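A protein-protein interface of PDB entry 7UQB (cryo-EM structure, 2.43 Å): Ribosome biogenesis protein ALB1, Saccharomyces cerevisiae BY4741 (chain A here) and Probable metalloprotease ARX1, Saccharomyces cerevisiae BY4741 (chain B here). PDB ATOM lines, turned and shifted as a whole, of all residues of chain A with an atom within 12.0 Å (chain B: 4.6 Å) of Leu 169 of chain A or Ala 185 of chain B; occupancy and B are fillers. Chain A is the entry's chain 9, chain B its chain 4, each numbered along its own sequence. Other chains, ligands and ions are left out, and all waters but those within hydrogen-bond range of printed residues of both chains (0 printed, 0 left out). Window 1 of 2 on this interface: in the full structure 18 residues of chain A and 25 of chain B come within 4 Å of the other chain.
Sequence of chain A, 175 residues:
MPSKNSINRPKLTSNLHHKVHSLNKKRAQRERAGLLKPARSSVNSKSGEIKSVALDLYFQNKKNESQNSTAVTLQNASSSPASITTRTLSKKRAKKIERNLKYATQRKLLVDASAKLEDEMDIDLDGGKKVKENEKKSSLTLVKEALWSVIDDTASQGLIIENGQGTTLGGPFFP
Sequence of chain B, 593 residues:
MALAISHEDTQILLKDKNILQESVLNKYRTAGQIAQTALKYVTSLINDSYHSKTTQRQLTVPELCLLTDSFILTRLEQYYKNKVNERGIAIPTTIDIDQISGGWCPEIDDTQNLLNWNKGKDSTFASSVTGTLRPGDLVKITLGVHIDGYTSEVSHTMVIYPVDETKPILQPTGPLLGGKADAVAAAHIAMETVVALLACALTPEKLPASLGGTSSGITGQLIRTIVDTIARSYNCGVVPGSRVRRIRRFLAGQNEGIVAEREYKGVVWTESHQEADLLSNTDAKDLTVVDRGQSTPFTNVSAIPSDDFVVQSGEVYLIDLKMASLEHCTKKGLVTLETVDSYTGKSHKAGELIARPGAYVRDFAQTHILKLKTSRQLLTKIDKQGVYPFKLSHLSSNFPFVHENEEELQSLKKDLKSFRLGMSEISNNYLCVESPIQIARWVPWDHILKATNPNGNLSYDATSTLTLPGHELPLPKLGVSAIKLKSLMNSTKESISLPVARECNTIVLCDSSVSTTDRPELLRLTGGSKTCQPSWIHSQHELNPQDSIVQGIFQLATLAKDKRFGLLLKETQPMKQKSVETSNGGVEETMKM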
ATOM      1  N   GLN A 165      22.460  22.707   3.150  1.00  0.00           N
ATOM      2  CA  GLN A 165      21.726  23.913   2.783  1.00  0.00           C
ATOM      3  C   GLN A 165      21.172  23.817   1.365  1.00  0.00           C
ATOM      4  O   GLN A 165      20.528  22.830   1.004  1.00  0.00           O
ATOM      5  CB  GLN A 165      22.624  25.145   2.914  1.00  0.00           C
ATOM      6  CG  GLN A 165      23.023  25.477   4.344  1.00  0.00           C
ATOM      7  CD  GLN A 165      21.892  26.100   5.141  1.00  0.00           C
ATOM      8  OE1 GLN A 165      20.886  26.536   4.581  1.00  0.00           O
ATOM      9  NE2 GLN A 165      22.056  26.151   6.459  1.00  0.00           N
ATOM     10  N   GLY A 166      21.425  24.850   0.566  1.00  0.00           N
ATOM     11  CA  GLY A 166      20.941  24.895  -0.799  1.00  0.00           C
ATOM     12  C   GLY A 166      20.652  26.306  -1.265  1.00  0.00           C
ATOM     13  O   GLY A 166      21.470  27.211  -1.075  1.00  0.00           O
ATOM     14  N   THR A 167      19.490  26.508  -1.883  1.00  0.00           N
ATOM     15  CA  THR A 167      19.070  27.839  -2.289  1.00  0.00           C
ATOM     16  C   THR A 167      17.560  27.946  -2.124  1.00  0.00           C
ATOM     17  O   THR A 167      16.844  26.941  -2.106  1.00  0.00           O
ATOM     18  CB  THR A 167      19.485  28.155  -3.735  1.00  0.00           C
ATOM     19  OG1 THR A 167      19.385  29.565  -3.966  1.00  0.00           O
ATOM     20  CG2 THR A 167      18.598  27.428  -4.725  1.00  0.00           C
ATOM     21  N   THR A 168      17.087  29.180  -1.981  1.00  0.00           N
ATOM     22  CA  THR A 168      15.663  29.437  -1.818  1.00  0.00           C
ATOM     23  C   THR A 168      15.333  30.792  -2.421  1.00  0.00           C
ATOM     24  O   THR A 168      15.951  31.801  -2.069  1.00  0.00           O
ATOM     25  CB  THR A 168      15.250  29.397  -0.342  1.00  0.00           C
ATOM     26  OG1 THR A 168      15.363  28.056   0.151  1.00  0.00           O
ATOM     27  CG2 THR A 168      13.813  29.872  -0.173  1.00  0.00           C
ATOM     28  N   LEU A 169      14.365  30.805  -3.332  1.00  0.00           N
ATOM     29  CA  LEU A 169      13.859  32.024  -3.937  1.00  0.00           C
ATOM     30  C   LEU A 169      12.390  32.186  -3.578  1.00  0.00           C
ATOM     31  O   LEU A 169      11.668  31.201  -3.392  1.00  0.00           O
ATOM     32  CB  LEU A 169      14.029  32.002  -5.460  1.00  0.00           C
ATOM     33  CG  LEU A 169      15.470  31.986  -5.972  1.00  0.00           C
ATOM     34  CD1 LEU A 169      15.513  31.666  -7.454  1.00  0.00           C
ATOM     35  CD2 LEU A 169      16.144  33.316  -5.692  1.00  0.00           C
ATOM     36  N   GLY A 170      11.954  33.436  -3.472  1.00  0.00           N
ATOM     37  CA  GLY A 170      10.576  33.718  -3.142  1.00  0.00           C
ATOM     38  C   GLY A 170      10.276  33.531  -1.667  1.00  0.00           C
ATOM     39  O   GLY A 170      11.163  33.369  -0.825  1.00  0.00           O
ATOM     40  N   GLY A 171       8.983  33.555  -1.359  1.00  0.00           N
ATOM     41  CA  GLY A 171       8.517  33.423   0.000  1.00  0.00           C
ATOM     42  C   GLY A 171       7.064  33.006   0.065  1.00  0.00           C
ATOM     43  O   GLY A 171       6.438  32.696  -0.952  1.00  0.00           O
ATOM     44  N   PRO A 172       6.489  33.003   1.270  1.00  0.00           N
ATOM     45  CA  PRO A 172       5.105  32.530   1.454  1.00  0.00           C
ATOM     46  C   PRO A 172       4.070  33.552   0.991  1.00  0.00           C
ATOM     47  O   PRO A 172       3.268  34.069   1.775  1.00  0.00           O
ATOM     48  CB  PRO A 172       5.049  32.278   2.966  1.00  0.00           C
ATOM     49  CG  PRO A 172       5.964  33.309   3.530  1.00  0.00           C
ATOM     50  CD  PRO A 172       7.089  33.460   2.536  1.00  0.00           C
ATOM     51  N   PHE A 173       4.080  33.844  -0.306  1.00  0.00           N
ATOM     52  CA  PHE A 173       3.164  34.819  -0.881  1.00  0.00           C
ATOM     53  C   PHE A 173       3.038  34.551  -2.372  1.00  0.00           C
ATOM     54  O   PHE A 173       3.930  33.969  -2.994  1.00  0.00           O
ATOM     55  CB  PHE A 173       3.638  36.257  -0.628  1.00  0.00           C
ATOM     56  CG  PHE A 173       4.862  36.642  -1.416  1.00  0.00           C
ATOM     57  CD1 PHE A 173       6.117  36.188  -1.042  1.00  0.00           C
ATOM     58  CD2 PHE A 173       4.756  37.465  -2.525  1.00  0.00           C
ATOM     59  CE1 PHE A 173       7.242  36.540  -1.764  1.00  0.00           C
ATOM     60  CE2 PHE A 173       5.878  37.822  -3.251  1.00  0.00           C
ATOM     61  CZ  PHE A 173       7.122  37.359  -2.870  1.00  0.00           C
ATOM     62  N   PHE A 174       1.916  34.996  -2.940  1.00  0.00           N
ATOM     63  CA  PHE A 174       1.709  34.913  -4.377  1.00  0.00           C
ATOM     64  C   PHE A 174       2.066  36.252  -5.000  1.00  0.00           C
ATOM     65  O   PHE A 174       1.376  37.248  -4.735  1.00  0.00           O
ATOM     66  CB  PHE A 174       0.262  34.546  -4.701  1.00  0.00           C
ATOM     67  CG  PHE A 174      -0.126  33.166  -4.263  1.00  0.00           C
ATOM     68  CD1 PHE A 174       0.422  32.051  -4.877  1.00  0.00           C
ATOM     69  CD2 PHE A 174      -1.050  32.980  -3.249  1.00  0.00           C
ATOM     70  CE1 PHE A 174       0.063  30.780  -4.481  1.00  0.00           C
ATOM     71  CE2 PHE A 174      -1.413  31.711  -2.848  1.00  0.00           C
ATOM     72  CZ  PHE A 174      -0.854  30.609  -3.465  1.00  0.00           C
ATOM     73  N   PRO A 175       3.128  36.337  -5.818  1.00  0.00           N
ATOM     74  CA  PRO A 175       3.544  37.577  -6.485  1.00  0.00           C
ATOM     75  C   PRO A 175       2.470  38.152  -7.405  1.00  0.00           C
ATOM     76  O   PRO A 175       1.731  39.037  -6.973  1.00  0.00           O
ATOM     77  CB  PRO A 175       4.770  37.142  -7.294  1.00  0.00           C
ATOM     78  CG  PRO A 175       5.292  35.950  -6.575  1.00  0.00           C
ATOM     79  CD  PRO A 175       4.082  35.241  -6.051  1.00  0.00           C
ATOM     80  N   ALA B 181      12.127  23.001  -9.306  1.00  0.00           N
ATOM     81  CA  ALA B 181      12.724  24.065  -8.506  1.00  0.00           C
ATOM     82  C   ALA B 181      14.162  24.336  -8.932  1.00  0.00           C
ATOM     83  O   ALA B 181      14.591  25.496  -8.986  1.00  0.00           O
ATOM     84  CB  ALA B 181      12.659  23.704  -7.022  1.00  0.00           C
ATOM     85  N   ASP B 182      14.919  23.276  -9.241  1.00  0.00           N
ATOM     86  CA  ASP B 182      16.280  23.458  -9.743  1.00  0.00           C
ATOM     87  C   ASP B 182      16.286  24.251 -11.043  1.00  0.00           C
ATOM     88  O   ASP B 182      17.116  25.148 -11.230  1.00  0.00           O
ATOM     89  CB  ASP B 182      16.958  22.104  -9.964  1.00  0.00           C
ATOM     90  CG  ASP B 182      17.051  21.276  -8.700  1.00  0.00           C
ATOM     91  OD1 ASP B 182      16.914  21.842  -7.599  1.00  0.00           O
ATOM     92  OD2 ASP B 182      17.273  20.051  -8.810  1.00  0.00           O
ATOM     93  N   ALA B 183      15.363  23.930 -11.953  1.00  0.00           N
ATOM     94  CA  ALA B 183      15.297  24.622 -13.236  1.00  0.00           C
ATOM     95  C   ALA B 183      14.914  26.086 -13.061  1.00  0.00           C
ATOM     96  O   ALA B 183      15.496  26.965 -13.710  1.00  0.00           O
ATOM     97  CB  ALA B 183      14.313  23.913 -14.162  1.00  0.00           C
ATOM     98  N   VAL B 184      13.939  26.366 -12.190  1.00  0.00           N
ATOM     99  CA  VAL B 184      13.541  27.751 -11.940  1.00  0.00           C
ATOM    100  C   VAL B 184      14.698  28.542 -11.343  1.00  0.00           C
ATOM    101  O   VAL B 184      14.980  29.673 -11.767  1.00  0.00           O
ATOM    102  CB  VAL B 184      12.293  27.797 -11.037  1.00  0.00           C
ATOM    103  CG1 VAL B 184      12.046  29.210 -10.536  1.00  0.00           C
ATOM    104  CG2 VAL B 184      11.080  27.294 -11.793  1.00  0.00           C
ATOM    105  N   ALA B 185      15.397  27.958 -10.364  1.00  0.00           N
ATOM    106  CA  ALA B 185      16.529  28.642  -9.746  1.00  0.00           C
ATOM    107  C   ALA B 185      17.642  28.899 -10.754  1.00  0.00           C
ATOM    108  O   ALA B 185      18.211  29.997 -10.790  1.00  0.00           O
ATOM    109  CB  ALA B 185      17.056  27.826  -8.569  1.00  0.00           C
ATOM    110  N   ALA B 186      17.956  27.902 -11.587  1.00  0.00           N
ATOM    111  CA  ALA B 186      19.010  28.068 -12.579  1.00  0.00           C
ATOM    112  C   ALA B 186      18.656  29.151 -13.588  1.00  0.00           C
ATOM    113  O   ALA B 186      19.493  30.002 -13.909  1.00  0.00           O
ATOM    114  CB  ALA B 186      19.277  26.742 -13.290  1.00  0.00           C
ATOM    115  N   ALA B 187      17.413  29.149 -14.081  1.00  0.00           N
ATOM    116  CA  ALA B 187      16.999  30.164 -15.045  1.00  0.00           C
ATOM    117  C   ALA B 187      17.045  31.562 -14.438  1.00  0.00           C
ATOM    118  O   ALA B 187      17.562  32.496 -15.061  1.00  0.00           O
ATOM    119  CB  ALA B 187      15.598  29.851 -15.570  1.00  0.00           C
ATOM    120  N   HIS B 188      16.541  31.718 -13.209  1.00  0.00           N
ATOM    121  CA  HIS B 188      16.518  33.031 -12.569  1.00  0.00           C
ATOM    122  C   HIS B 188      17.930  33.551 -12.310  1.00  0.00           C
ATOM    123  O   HIS B 188      18.244  34.715 -12.609  1.00  0.00           O
ATOM    124  CB  HIS B 188      15.724  32.954 -11.265  1.00  0.00           C
ATOM    125  CG  HIS B 188      15.681  34.241 -10.504  1.00  0.00           C
ATOM    126  ND1 HIS B 188      16.379  34.436  -9.331  1.00  0.00           N
ATOM    127  CD2 HIS B 188      15.022  35.399 -10.745  1.00  0.00           C
ATOM    128  CE1 HIS B 188      16.152  35.658  -8.885  1.00  0.00           C
ATOM    129  NE2 HIS B 188      15.332  36.264  -9.725  1.00  0.00           N
ATOM    130  N   ILE B 189      18.801  32.698 -11.768  1.00  0.00           N
ATOM    131  CA  ILE B 189      20.151  33.130 -11.428  1.00  0.00           C
ATOM    132  C   ILE B 189      20.961  33.408 -12.686  1.00  0.00           C
ATOM    133  O   ILE B 189      21.722  34.383 -12.742  1.00  0.00           O
ATOM    134  CB  ILE B 189      20.821  32.085 -10.518  1.00  0.00           C
ATOM    135  CG1 ILE B 189      20.135  32.084  -9.152  1.00  0.00           C
ATOM    136  CG2 ILE B 189      22.308  32.360 -10.366  1.00  0.00           C
ATOM    137  CD1 ILE B 189      20.614  31.009  -8.234  1.00  0.00           C
ATOM    138  N   TYR B 234      23.399  23.661 -10.992  1.00  0.00           N
ATOM    139  CA  TYR B 234      22.030  23.326 -10.619  1.00  0.00           C
ATOM    140  C   TYR B 234      21.526  22.047 -11.278  1.00  0.00           C
ATOM    141  O   TYR B 234      20.346  21.715 -11.126  1.00  0.00           O
ATOM    142  CB  TYR B 234      21.096  24.497 -10.929  1.00  0.00           C
ATOM    143  CG  TYR B 234      21.094  25.514  -9.817  1.00  0.00           C
ATOM    144  CD1 TYR B 234      20.436  25.254  -8.623  1.00  0.00           C
ATOM    145  CD2 TYR B 234      21.771  26.717  -9.943  1.00  0.00           C
ATOM    146  CE1 TYR B 234      20.438  26.167  -7.593  1.00  0.00           C
ATOM    147  CE2 TYR B 234      21.778  27.641  -8.915  1.00  0.00           C
ATOM    148  CZ  TYR B 234      21.108  27.357  -7.743  1.00  0.00           C
ATOM    149  OH  TYR B 234      21.107  28.262  -6.709  1.00  0.00           O
ATOM    150  N   PRO B 534      10.544  35.999  -8.574  1.00  0.00           N
ATOM    151  CA  PRO B 534      10.599  34.534  -8.497  1.00  0.00           C
ATOM    152  C   PRO B 534       9.593  33.966  -7.507  1.00  0.00           C
ATOM    153  O   PRO B 534       9.296  34.562  -6.469  1.00  0.00           O
ATOM    154  CB  PRO B 534      12.036  34.258  -8.046  1.00  0.00           C
ATOM    155  CG  PRO B 534      12.438  35.497  -7.319  1.00  0.00           C
ATOM    156  CD  PRO B 534      11.766  36.626  -8.043  1.00  0.00           C
ATOM    157  N   SER B 535       9.069  32.792  -7.846  1.00  0.00           N
ATOM    158  CA  SER B 535       8.101  32.103  -7.010  1.00  0.00           C
ATOM    159  C   SER B 535       8.809  31.347  -5.885  1.00  0.00           C
ATOM    160  O   SER B 535      10.028  31.166  -5.890  1.00  0.00           O
ATOM    161  CB  SER B 535       7.256  31.147  -7.851  1.00  0.00           C
ATOM    162  OG  SER B 535       6.580  31.839  -8.886  1.00  0.00           O
ATOM    163  N   TRP B 536       8.020  30.897  -4.910  1.00  0.00           N
ATOM    164  CA  TRP B 536       8.556  30.219  -3.730  1.00  0.00           C
ATOM    165  C   TRP B 536       9.045  28.833  -4.125  1.00  0.00           C
ATOM    166  O   TRP B 536       8.251  27.908  -4.310  1.00  0.00           O
ATOM    167  CB  TRP B 536       7.501  30.132  -2.633  1.00  0.00           C
ATOM    168  CG  TRP B 536       8.057  29.711  -1.297  1.00  0.00           C
ATOM    169  CD1 TRP B 536       9.373  29.626  -0.946  1.00  0.00           C
ATOM    170  CD2 TRP B 536       7.310  29.320  -0.139  1.00  0.00           C
ATOM    171  NE1 TRP B 536       9.492  29.207   0.356  1.00  0.00           N
ATOM    172  CE2 TRP B 536       8.238  29.013   0.874  1.00  0.00           C
ATOM    173  CE3 TRP B 536       5.944  29.199   0.140  1.00  0.00           C
ATOM    174  CZ2 TRP B 536       7.848  28.593   2.144  1.00  0.00           C
ATOM    175  CZ3 TRP B 536       5.558  28.782   1.400  1.00  0.00           C
ATOM    176  CH2 TRP B 536       6.506  28.485   2.387  1.00  0.00           C
ATOM    177  N   ILE B 537      10.362  28.682  -4.247  1.00  0.00           N
ATOM    178  CA  ILE B 537      10.985  27.406  -4.561  1.00  0.00           C
ATOM    179  C   ILE B 537      12.057  27.123  -3.520  1.00  0.00           C
ATOM    180  O   ILE B 537      12.565  28.026  -2.851  1.00  0.00           O
ATOM    181  CB  ILE B 537      11.601  27.374  -5.978  1.00  0.00           C
ATOM    182  CG1 ILE B 537      12.840  28.267  -6.039  1.00  0.00           C
ATOM    183  CG2 ILE B 537      10.583  27.801  -7.027  1.00  0.00           C
ATOM    184  CD1 ILE B 537      13.582  28.187  -7.341  1.00  0.00           C
ATOM    185  N   SER B 539      15.523  24.641  -3.651  1.00  0.00           N
ATOM    186  CA  SER B 539      16.372  23.733  -4.406  1.00  0.00           C
ATOM    187  C   SER B 539      17.550  23.310  -3.542  1.00  0.00           C
ATOM    188  O   SER B 539      18.237  24.159  -2.966  1.00  0.00           O
ATOM    189  CB  SER B 539      16.866  24.395  -5.696  1.00  0.00           C
ATOM    190  OG  SER B 539      17.815  23.577  -6.358  1.00  0.00           O
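Hydrophobic or aromatic side chains of chain B that line the printed part of chain A: His 188, Tyr 234, Pro 534, Trp 536 and Ile 537.
Of the 11 printed residues of chain A, 7 touch a printed residue of chain B.
Printed residues of chain A that touch a printed residue of chain B: Gly 166, Thr 167, Thr 168, Leu 169, Gly 170, Gly 171 and Pro 172.
Among the printed residues, 14 pairs touch across the chains.
Among the printed residues, no Asp or Glu carboxylate lies within 4 Å of a Lys or Arg side-chain nitrogen of the other chain.
The side-chain hydroxyl (OG1) of Thr 167 of chain A sits close to the side-chain hydroxyl (OH) of Tyr 234 of chain B (3.5 Å).
N of Ile 537 of chain B sits at hydrogen-bond distance from O of Leu 169 of chain A (3.0 Å).
The backbone carbonyl oxygen of Leu 169 of chain A lies close to the backbone carbonyl oxygen of Ser 535 of chain B, 3.0 Å away.
The backbone carbonyl oxygen (O) of Ser 539 of chain B is in hydrogen-bond range of the backbone NH (N) of Thr 167 of chain A (2.9 Å).
Among the printed residues, pairs that only touch across the chains: Gly 171 of chain A with Trp 536 of chain B (3.2 Å), Leu 169 of chain A with Trp 536 of chain B (3.3 Å), Leu 169 of chain A with His 188 of chain B (3.5 Å), Thr 168 of chain A with Ile 537 of chain B (3.5 Å), Gly 166 of chain A with Ser 539 of chain B (3.5 Å), Gly 170 of chain A with Pro 534 of chain B (3.7 Å), Pro 172 of chain A with Trp 536 of chain B (3.7 Å), Gly 170 of chain A with Ser 535 of chain B (3.8 Å), Leu 169 of chain A with Ala 185 of chain B (3.9 Å) and Leu 169 of chain A with Pro 534 of chain B (3.97 Å).
Leu 169 of chain A touches just these residues of chain B: Ala 185 (3.9 Å), His 188 (3.5 Å), Pro 534 (3.97 Å), Ser 535 (3.0 Å), Trp 536 (3.3 Å) and Ile 537 (3.0 Å).
Ala 185 of chain B touches just one residue of chain A: Leu 169 (3.9 Å).
No residue of chain A comes within 4 Å of Ala 181 of chain B.
No residue of chain A comes within 4 Å of Asp 182 of chain B.
Ala 186 of chain B touches none of the printed residues of chain A.
No residue of chain A comes within 4 Å of Ala 187 of chain B.
His 188 of chain B touches just one residue of chain A: Leu 169 (3.5 Å).
No residue of chain A comes within 4 Å of Ile 189 of chain B.
Tyr 234 of chain B touches one residue of chain A.
Of chain A, only Leu 169 (3.97 Å) and Gly 170 (3.7 Å) come within 4 Å of Pro 534 of chain B.
Of the printed residues of chain B, Gly 171 of chain A touches Trp 536 (3.2 Å).
Of the printed residues of chain B, Thr 167 of chain A touches Tyr 234 and Ser 539.
Of the printed residues of chain B, Gly 166 of chain A touches Ser 539 (3.5 Å).
Printed residues of chain A within 4 Å of Trp 536 of chain B: Leu 169 (3.3 Å), Gly 171 (3.2 Å) and Pro 172 (3.7 Å).
Printed residues of chain B within 4 Å of Pro 172 of chain A: Trp 536.
Pro 175 of chain A touches none of the printed residues of chain B.
Phe 173 of chain A touches none of the printed residues of chain B.
The nearest printed residue of chain B that does not touch Leu 169 of chain A is Val 184 of chain B (4.8 Å).
The nearest residue of chain A that does not touch Ala 185 of chain B is Thr 167 of chain A (4.2 Å).
The nearest printed residue of chain B that does not touch Gly 166 of chain A is Tyr 234 of chain B (5.7 Å).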
